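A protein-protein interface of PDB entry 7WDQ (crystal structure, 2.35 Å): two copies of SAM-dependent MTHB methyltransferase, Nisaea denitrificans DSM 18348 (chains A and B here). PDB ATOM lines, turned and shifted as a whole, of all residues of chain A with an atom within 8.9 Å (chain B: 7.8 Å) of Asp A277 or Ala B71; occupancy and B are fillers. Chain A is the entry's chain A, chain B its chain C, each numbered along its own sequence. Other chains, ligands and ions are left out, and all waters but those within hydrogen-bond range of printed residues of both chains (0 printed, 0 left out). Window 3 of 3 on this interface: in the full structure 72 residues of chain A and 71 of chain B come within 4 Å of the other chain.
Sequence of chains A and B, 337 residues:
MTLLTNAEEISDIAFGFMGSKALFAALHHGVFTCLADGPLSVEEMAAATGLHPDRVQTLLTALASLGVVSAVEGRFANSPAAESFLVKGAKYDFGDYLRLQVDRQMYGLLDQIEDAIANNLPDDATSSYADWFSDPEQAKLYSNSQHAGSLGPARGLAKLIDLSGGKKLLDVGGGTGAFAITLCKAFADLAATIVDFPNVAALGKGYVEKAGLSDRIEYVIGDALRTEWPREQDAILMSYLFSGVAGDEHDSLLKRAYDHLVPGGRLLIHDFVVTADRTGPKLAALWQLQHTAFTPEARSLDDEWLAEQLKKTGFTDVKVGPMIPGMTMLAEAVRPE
No position is printed for both chains.
Among the printed residues, pairs that only touch across the chains: Thr A279 with Ser B65, Arg A278 with Ala B64, Leu A3 with Ser B70, Leu A3 with Val B69, Asp A277 with Ala B71 and Arg A278 with Ala B71.
The side-chain hydroxyl (OG1) of Thr B61 sits at hydrogen-bond distance from the guanidinium group (NH1) of Arg A278 (3.0 Å).
Ala A276 touches none of the printed residues of chain B. Of the printed residues of chain B, Asp A277 touches Ala B71 (3.9 Å). Printed residues of chain B within 4 Å of Thr A279: Ser B65. Gly A280 touches none of the printed residues of chain B. Pro A281 touches none of the printed residues of chain B. Of the printed residues of chain A, Thr B61 touches Arg A278. Of the printed residues of chain A, Ala B64 touches Arg A278. Of the printed residues of chain A, Val B69 touches Leu A3. Ser B70 touches one residue of chain A. Ala B71 touches just these residues of chain A: Asp A277 and Arg A278. No residue of chain A comes within 4 Å of Val B72. The nearest residue of chain B that does not touch Asp A277 is Val B72 (5.7 Å). The nearest residue of chain A that does not touch Ala B71 is Thr A279 (4.7 Å). The nearest printed residue of chain A that does not touch Ser B65 is Gly A280 (4.05 Å).
Printed residues of chain B that touch a printed residue of chain A: Thr B61, Ala B64, Ser B65, Val B69, Ser B70 and Ala B71. Hydrophobic or aromatic side chains of chain B within 4 Å of the printed part of chain A: Ala B64 and Ala B71. Of the 14 printed residues of chain A, 4 touch a printed residue of chain B. Printed residues of chain A that touch a printed residue of chain B: Leu A3, Asp A277, Arg A278 and Thr A279. Hydrophobic or aromatic side chains of chain A within 4 Å of the printed part of chain B: Leu A3.
The side-chain carboxylate of Asp A277 is in hydrogen-bond range of the side-chain hydroxyl of Thr A275, 2.5 Å away. The backbone NH (N) of Ser B70 sits at hydrogen-bond distance from the backbone carbonyl oxygen (O) of Ala B77 (2.9 Å). The guanidinium group of Arg A278 lies within salt-bridge range of the side-chain carboxylate of Asp A302. OD1 of Asp A277 lies close to N of Thr A279 (3.4 Å).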
ATOM      1  N   THR A   2       7.635  24.138  14.233  1.00  0.00           N
ATOM      2  CA  THR A   2       8.722  24.945  13.689  1.00  0.00           C
ATOM      3  C   THR A   2       8.730  26.319  14.321  1.00  0.00           C
ATOM      4  O   THR A   2       7.714  26.788  14.828  1.00  0.00           O
ATOM      5  CB  THR A   2       8.608  25.140  12.171  1.00  0.00           C
ATOM      6  OG1 THR A   2       7.303  25.641  11.854  1.00  0.00           O
ATOM      7  CG2 THR A   2       8.839  23.821  11.435  1.00  0.00           C
ATOM      8  N   LEU A   3       9.895  26.951  14.293  1.00  0.00           N
ATOM      9  CA  LEU A   3      10.063  28.300  14.783  1.00  0.00           C
ATOM     10  C   LEU A   3      10.868  28.951  13.681  1.00  0.00           C
ATOM     11  O   LEU A   3      11.916  28.439  13.302  1.00  0.00           O
ATOM     12  CB  LEU A   3      10.851  28.291  16.088  1.00  0.00           C
ATOM     13  CG  LEU A   3      10.607  29.386  17.112  1.00  0.00           C
ATOM     14  CD1 LEU A   3       9.168  29.290  17.566  1.00  0.00           C
ATOM     15  CD2 LEU A   3      11.559  29.212  18.281  1.00  0.00           C
ATOM     16  N   VAL A 273     -11.584  25.350  17.691  1.00  0.00           N
ATOM     17  CA  VAL A 273     -11.007  25.257  19.020  1.00  0.00           C
ATOM     18  C   VAL A 273      -9.526  24.925  18.961  1.00  0.00           C
ATOM     19  O   VAL A 273      -9.127  23.935  18.355  1.00  0.00           O
ATOM     20  CB  VAL A 273     -11.714  24.190  19.866  1.00  0.00           C
ATOM     21  CG1 VAL A 273     -11.189  24.223  21.311  1.00  0.00           C
ATOM     22  CG2 VAL A 273     -13.220  24.390  19.808  1.00  0.00           C
ATOM     23  N   VAL A 274      -8.708  25.743  19.603  1.00  0.00           N
ATOM     24  CA  VAL A 274      -7.302  25.411  19.693  1.00  0.00           C
ATOM     25  C   VAL A 274      -6.995  24.508  20.895  1.00  0.00           C
ATOM     26  O   VAL A 274      -7.790  24.399  21.836  1.00  0.00           O
ATOM     27  CB  VAL A 274      -6.438  26.679  19.705  1.00  0.00           C
ATOM     28  CG1 VAL A 274      -6.693  27.485  18.435  1.00  0.00           C
ATOM     29  CG2 VAL A 274      -6.713  27.509  20.954  1.00  0.00           C
ATOM     30  N   THR A 275      -5.851  23.833  20.838  1.00  0.00           N
ATOM     31  CA  THR A 275      -5.371  23.034  21.957  1.00  0.00           C
ATOM     32  C   THR A 275      -4.859  23.964  23.044  1.00  0.00           C
ATOM     33  O   THR A 275      -4.404  25.068  22.758  1.00  0.00           O
ATOM     34  CB  THR A 275      -4.244  22.087  21.523  1.00  0.00           C
ATOM     35  OG1 THR A 275      -3.241  22.840  20.843  1.00  0.00           O
ATOM     36  CG2 THR A 275      -4.783  21.020  20.578  1.00  0.00           C
ATOM     37  N   ALA A 276      -4.945  23.519  24.292  1.00  0.00           N
ATOM     38  CA  ALA A 276      -4.581  24.359  25.431  1.00  0.00           C
ATOM     39  C   ALA A 276      -3.125  24.842  25.433  1.00  0.00           C
ATOM     40  O   ALA A 276      -2.789  25.820  26.113  1.00  0.00           O
ATOM     41  CB  ALA A 276      -4.891  23.646  26.726  1.00  0.00           C
ATOM     42  N   ASP A 277      -2.258  24.166  24.685  1.00  0.00           N
ATOM     43  CA  ASP A 277      -0.861  24.593  24.610  1.00  0.00           C
ATOM     44  C   ASP A 277      -0.705  25.776  23.648  1.00  0.00           C
ATOM     45  O   ASP A 277       0.353  26.414  23.588  1.00  0.00           O
ATOM     46  CB  ASP A 277       0.075  23.431  24.240  1.00  0.00           C
ATOM     47  CG  ASP A 277      -0.162  22.893  22.830  1.00  0.00           C
ATOM     48  OD1 ASP A 277      -1.174  23.270  22.197  1.00  0.00           O
ATOM     49  OD2 ASP A 277       0.666  22.075  22.358  1.00  0.00           O
ATOM     50  N   ARG A 278      -1.793  26.080  22.950  1.00  0.00           N
ATOM     51  CA  ARG A 278      -1.914  27.259  22.108  1.00  0.00           C
ATOM     52  C   ARG A 278      -0.939  27.242  20.967  1.00  0.00           C
ATOM     53  O   ARG A 278      -0.320  28.236  20.645  1.00  0.00           O
ATOM     54  CB  ARG A 278      -1.747  28.520  22.931  1.00  0.00           C
ATOM     55  CG  ARG A 278      -2.642  28.541  24.143  1.00  0.00           C
ATOM     56  CD  ARG A 278      -3.459  29.800  24.198  1.00  0.00           C
ATOM     57  NE  ARG A 278      -4.803  29.540  24.678  1.00  0.00           N
ATOM     58  CZ  ARG A 278      -5.904  29.894  24.036  1.00  0.00           C
ATOM     59  NH1 ARG A 278      -5.828  30.520  22.879  1.00  0.00           N
ATOM     60  NH2 ARG A 278      -7.077  29.624  24.560  1.00  0.00           N
ATOM     61  N   THR A 279      -0.830  26.087  20.349  1.00  0.00           N
ATOM     62  CA  THR A 279       0.183  25.851  19.354  1.00  0.00           C
ATOM     63  C   THR A 279      -0.458  25.608  17.995  1.00  0.00           C
ATOM     64  O   THR A 279       0.215  25.558  16.986  1.00  0.00           O
ATOM     65  CB  THR A 279       1.121  24.723  19.856  1.00  0.00           C
ATOM     66  OG1 THR A 279       2.466  25.190  19.868  1.00  0.00           O
ATOM     67  CG2 THR A 279       1.017  23.423  19.063  1.00  0.00           C
ATOM     68  N   GLY A 280      -1.771  25.470  18.005  1.00  0.00           N
ATOM     69  CA  GLY A 280      -2.540  25.129  16.836  1.00  0.00           C
ATOM     70  C   GLY A 280      -3.810  24.475  17.327  1.00  0.00           C
ATOM     71  O   GLY A 280      -4.056  24.572  18.501  1.00  0.00           O
ATOM     72  N   PRO A 281      -4.663  23.761  16.457  1.00  0.00           N
ATOM     73  CA  PRO A 281      -4.258  23.752  15.040  1.00  0.00           C
ATOM     74  C   PRO A 281      -4.328  25.110  14.349  1.00  0.00           C
ATOM     75  O   PRO A 281      -5.103  25.971  14.703  1.00  0.00           O
ATOM     76  CB  PRO A 281      -5.225  22.775  14.392  1.00  0.00           C
ATOM     77  CG  PRO A 281      -6.454  22.899  15.169  1.00  0.00           C
ATOM     78  CD  PRO A 281      -5.929  22.874  16.546  1.00  0.00           C
ATOM     79  N   ASP A 302     -10.170  27.223  23.810  1.00  0.00           N
ATOM     80  CA  ASP A 302      -9.263  26.079  23.824  1.00  0.00           C
ATOM     81  C   ASP A 302      -9.944  24.881  24.455  1.00  0.00           C
ATOM     82  O   ASP A 302     -10.891  25.041  25.224  1.00  0.00           O
ATOM     83  CB  ASP A 302      -7.962  26.376  24.556  1.00  0.00           C
ATOM     84  CG  ASP A 302      -8.159  26.550  26.049  1.00  0.00           C
ATOM     85  OD1 ASP A 302      -8.188  25.524  26.782  1.00  0.00           O
ATOM     86  OD2 ASP A 302      -8.280  27.723  26.484  1.00  0.00           O
ATOM     87  N   ASP A 303      -9.434  23.687  24.144  1.00  0.00           N
ATOM     88  CA  ASP A 303     -10.119  22.444  24.481  1.00  0.00           C
ATOM     89  C   ASP A 303     -10.320  22.177  25.971  1.00  0.00           C
ATOM     90  O   ASP A 303     -11.338  21.606  26.361  1.00  0.00           O
ATOM     91  CB  ASP A 303      -9.513  21.214  23.759  1.00  0.00           C
ATOM     92  CG  ASP A 303      -8.037  20.973  24.090  1.00  0.00           C
ATOM     93  OD1 ASP A 303      -7.400  21.783  24.810  1.00  0.00           O
ATOM     94  OD2 ASP A 303      -7.498  19.961  23.589  1.00  0.00           O
ATOM     95  N   GLU A 304      -9.379  22.573  26.816  1.00  0.00           N
ATOM     96  CA  GLU A 304      -9.549  22.205  28.210  1.00  0.00           C
ATOM     97  C   GLU A 304     -10.361  23.221  28.997  1.00  0.00           C
ATOM     98  O   GLU A 304     -11.016  22.869  29.971  1.00  0.00           O
ATOM     99  CB  GLU A 304      -8.230  21.822  28.887  1.00  0.00           C
ATOM    100  CG  GLU A 304      -7.216  22.918  29.028  1.00  0.00           C
ATOM    101  CD  GLU A 304      -5.880  22.400  29.581  1.00  0.00           C
ATOM    102  OE1 GLU A 304      -5.365  21.360  29.078  1.00  0.00           O
ATOM    103  OE2 GLU A 304      -5.353  23.037  30.523  1.00  0.00           O
ATOM    104  N   LEU B  60      -1.771  36.105  19.557  1.00  0.00           N
ATOM    105  CA  LEU B  60      -0.560  35.360  19.871  1.00  0.00           C
ATOM    106  C   LEU B  60      -0.673  33.873  19.511  1.00  0.00           C
ATOM    107  O   LEU B  60       0.295  33.268  19.044  1.00  0.00           O
ATOM    108  CB  LEU B  60      -0.187  35.548  21.347  1.00  0.00           C
ATOM    109  CG  LEU B  60       0.598  36.835  21.624  1.00  0.00           C
ATOM    110  CD1 LEU B  60       2.067  36.656  21.333  1.00  0.00           C
ATOM    111  CD2 LEU B  60       0.062  37.967  20.777  1.00  0.00           C
ATOM    112  N   THR B  61      -1.857  33.298  19.713  1.00  0.00           N
ATOM    113  CA  THR B  61      -2.083  31.896  19.370  1.00  0.00           C
ATOM    114  C   THR B  61      -1.969  31.686  17.856  1.00  0.00           C
ATOM    115  O   THR B  61      -1.325  30.739  17.397  1.00  0.00           O
ATOM    116  CB  THR B  61      -3.425  31.376  19.913  1.00  0.00           C
ATOM    117  OG1 THR B  61      -3.376  31.344  21.347  1.00  0.00           O
ATOM    118  CG2 THR B  61      -3.706  29.968  19.400  1.00  0.00           C
ATOM    119  N   LEU B  63      -0.199  33.559  15.765  1.00  0.00           N
ATOM    120  CA  LEU B  63       1.216  33.707  15.462  1.00  0.00           C
ATOM    121  C   LEU B  63       2.042  32.471  15.864  1.00  0.00           C
ATOM    122  O   LEU B  63       2.971  32.086  15.154  1.00  0.00           O
ATOM    123  CB  LEU B  63       1.772  34.935  16.180  1.00  0.00           C
ATOM    124  CG  LEU B  63       1.258  36.276  15.663  1.00  0.00           C
ATOM    125  CD1 LEU B  63       1.849  37.441  16.473  1.00  0.00           C
ATOM    126  CD2 LEU B  63       1.625  36.388  14.192  1.00  0.00           C
ATOM    127  N   ALA B  64       1.716  31.857  17.000  1.00  0.00           N
ATOM    128  CA  ALA B  64       2.482  30.711  17.467  1.00  0.00           C
ATOM    129  C   ALA B  64       2.280  29.543  16.524  1.00  0.00           C
ATOM    130  O   ALA B  64       3.215  28.791  16.265  1.00  0.00           O
ATOM    131  CB  ALA B  64       2.078  30.326  18.895  1.00  0.00           C
ATOM    132  N   SER B  65       1.063  29.409  15.993  1.00  0.00           N
ATOM    133  CA  SER B  65       0.734  28.333  15.054  1.00  0.00           C
ATOM    134  C   SER B  65       1.392  28.537  13.686  1.00  0.00           C
ATOM    135  O   SER B  65       1.414  27.625  12.855  1.00  0.00           O
ATOM    136  CB  SER B  65      -0.783  28.206  14.881  1.00  0.00           C
ATOM    137  OG  SER B  65      -1.310  29.261  14.088  1.00  0.00           O
ATOM    138  N   VAL B  68       5.838  32.069  14.272  1.00  0.00           N
ATOM    139  CA  VAL B  68       6.442  33.390  14.359  1.00  0.00           C
ATOM    140  C   VAL B  68       6.873  33.708  15.794  1.00  0.00           C
ATOM    141  O   VAL B  68       7.858  34.403  16.019  1.00  0.00           O
ATOM    142  CB  VAL B  68       5.522  34.489  13.777  1.00  0.00           C
ATOM    143  CG1 VAL B  68       6.262  35.822  13.706  1.00  0.00           C
ATOM    144  CG2 VAL B  68       5.029  34.082  12.403  1.00  0.00           C
ATOM    145  N   VAL B  69       6.127  33.198  16.762  1.00  0.00           N
ATOM    146  CA  VAL B  69       6.567  33.229  18.149  1.00  0.00           C
ATOM    147  C   VAL B  69       6.457  31.818  18.685  1.00  0.00           C
ATOM    148  O   VAL B  69       5.816  30.970  18.084  1.00  0.00           O
ATOM    149  CB  VAL B  69       5.678  34.106  19.034  1.00  0.00           C
ATOM    150  CG1 VAL B  69       5.588  35.522  18.470  1.00  0.00           C
ATOM    151  CG2 VAL B  69       4.316  33.483  19.165  1.00  0.00           C
ATOM    152  N   SER B  70       7.069  31.586  19.832  1.00  0.00           N
ATOM    153  CA  SER B  70       7.011  30.297  20.492  1.00  0.00           C
ATOM    154  C   SER B  70       5.957  30.429  21.553  1.00  0.00           C
ATOM    155  O   SER B  70       5.637  31.543  21.969  1.00  0.00           O
ATOM    156  CB  SER B  70       8.351  29.974  21.156  1.00  0.00           C
ATOM    157  OG  SER B  70       8.668  30.971  22.116  1.00  0.00           O
ATOM    158  N   ALA B  71       5.419  29.298  22.001  1.00  0.00           N
ATOM    159  CA  ALA B  71       4.426  29.298  23.062  1.00  0.00           C
ATOM    160  C   ALA B  71       4.818  28.260  24.093  1.00  0.00           C
ATOM    161  O   ALA B  71       4.713  27.066  23.831  1.00  0.00           O
ATOM    162  CB  ALA B  71       3.039  28.992  22.492  1.00  0.00           C
ATOM    163  N   VAL B  72       5.254  28.712  25.267  1.00  0.00           N
ATOM    164  CA  VAL B  72       5.769  27.806  26.293  1.00  0.00           C
ATOM    165  C   VAL B  72       5.336  28.211  27.698  1.00  0.00           C
ATOM    166  O   VAL B  72       5.637  29.312  28.145  1.00  0.00           O
ATOM    167  CB  VAL B  72       7.326  27.751  26.272  1.00  0.00           C
ATOM    168  CG1 VAL B  72       7.833  26.676  27.222  1.00  0.00           C
ATOM    169  CG2 VAL B  72       7.862  27.509  24.852  1.00  0.00           C
ATOM    170  N   GLU B  73       4.646  27.309  28.391  1.00  0.00           N
ATOM    171  CA  GLU B  73       4.194  27.549  29.763  1.00  0.00           C
ATOM    172  C   GLU B  73       3.352  28.807  29.922  1.00  0.00           C
ATOM    173  O   GLU B  73       3.560  29.583  30.851  1.00  0.00           O
ATOM    174  CB  GLU B  73       5.381  27.633  30.712  1.00  0.00           C
ATOM    175  CG  GLU B  73       6.188  26.346  30.811  1.00  0.00           C
ATOM    176  CD  GLU B  73       5.346  25.150  31.235  1.00  0.00           C
ATOM    177  OE1 GLU B  73       5.891  24.025  31.261  1.00  0.00           O
ATOM    178  OE2 GLU B  73       4.146  25.331  31.546  1.00  0.00           O
ATOM    179  N   GLY B  74       2.398  29.003  29.024  1.00  0.00           N
ATOM    180  CA  GLY B  74       1.596  30.210  29.038  1.00  0.00           C
ATOM    181  C   GLY B  74       2.407  31.467  28.772  1.00  0.00           C
ATOM    182  O   GLY B  74       1.955  32.577  29.076  1.00  0.00           O
ATOM    183  N   ARG B  75       3.607  31.306  28.211  1.00  0.00           N
ATOM    184  CA  ARG B  75       4.399  32.466  27.811  1.00  0.00           C
ATOM    185  C   ARG B  75       4.755  32.469  26.330  1.00  0.00           C
ATOM    186  O   ARG B  75       4.928  31.425  25.695  1.00  0.00           O
ATOM    187  CB  ARG B  75       5.664  32.614  28.652  1.00  0.00           C
ATOM    188  CG  ARG B  75       5.415  32.898  30.119  1.00  0.00           C
ATOM    189  CD  ARG B  75       6.526  33.785  30.655  1.00  0.00           C
ATOM    190  NE  ARG B  75       6.894  33.457  32.030  1.00  0.00           N
ATOM    191  CZ  ARG B  75       6.447  34.109  33.102  1.00  0.00           C
ATOM    192  NH1 ARG B  75       5.605  35.140  32.967  1.00  0.00           N
ATOM    193  NH2 ARG B  75       6.849  33.729  34.313  1.00  0.00           N
ATOM    194  N   PHE B  76       4.867  33.668  25.782  1.00  0.00           N
ATOM    195  CA  PHE B  76       5.171  33.816  24.375  1.00  0.00           C
ATOM    196  C   PHE B  76       6.508  34.512  24.211  1.00  0.00           C
ATOM    197  O   PHE B  76       6.842  35.398  24.995  1.00  0.00           O
ATOM    198  CB  PHE B  76       4.061  34.606  23.676  1.00  0.00           C
ATOM    199  CG  PHE B  76       2.757  33.870  23.589  1.00  0.00           C
ATOM    200  CD1 PHE B  76       2.502  33.012  22.537  1.00  0.00           C
ATOM    201  CD2 PHE B  76       1.784  34.039  24.557  1.00  0.00           C
ATOM    202  CE1 PHE B  76       1.300  32.342  22.442  1.00  0.00           C
ATOM    203  CE2 PHE B  76       0.574  33.371  24.474  1.00  0.00           C
ATOM    204  CZ  PHE B  76       0.330  32.523  23.411  1.00  0.00           C
ATOM    205  N   ALA B  77       7.267  34.114  23.191  1.00  0.00           N
ATOM    206  CA  ALA B  77       8.539  34.757  22.909  1.00  0.00           C
ATOM    207  C   ALA B  77       8.765  34.898  21.411  1.00  0.00           C
ATOM    208  O   ALA B  77       8.200  34.146  20.623  1.00  0.00           O
ATOM    209  CB  ALA B  77       9.686  33.984  23.565  1.00  0.00           C
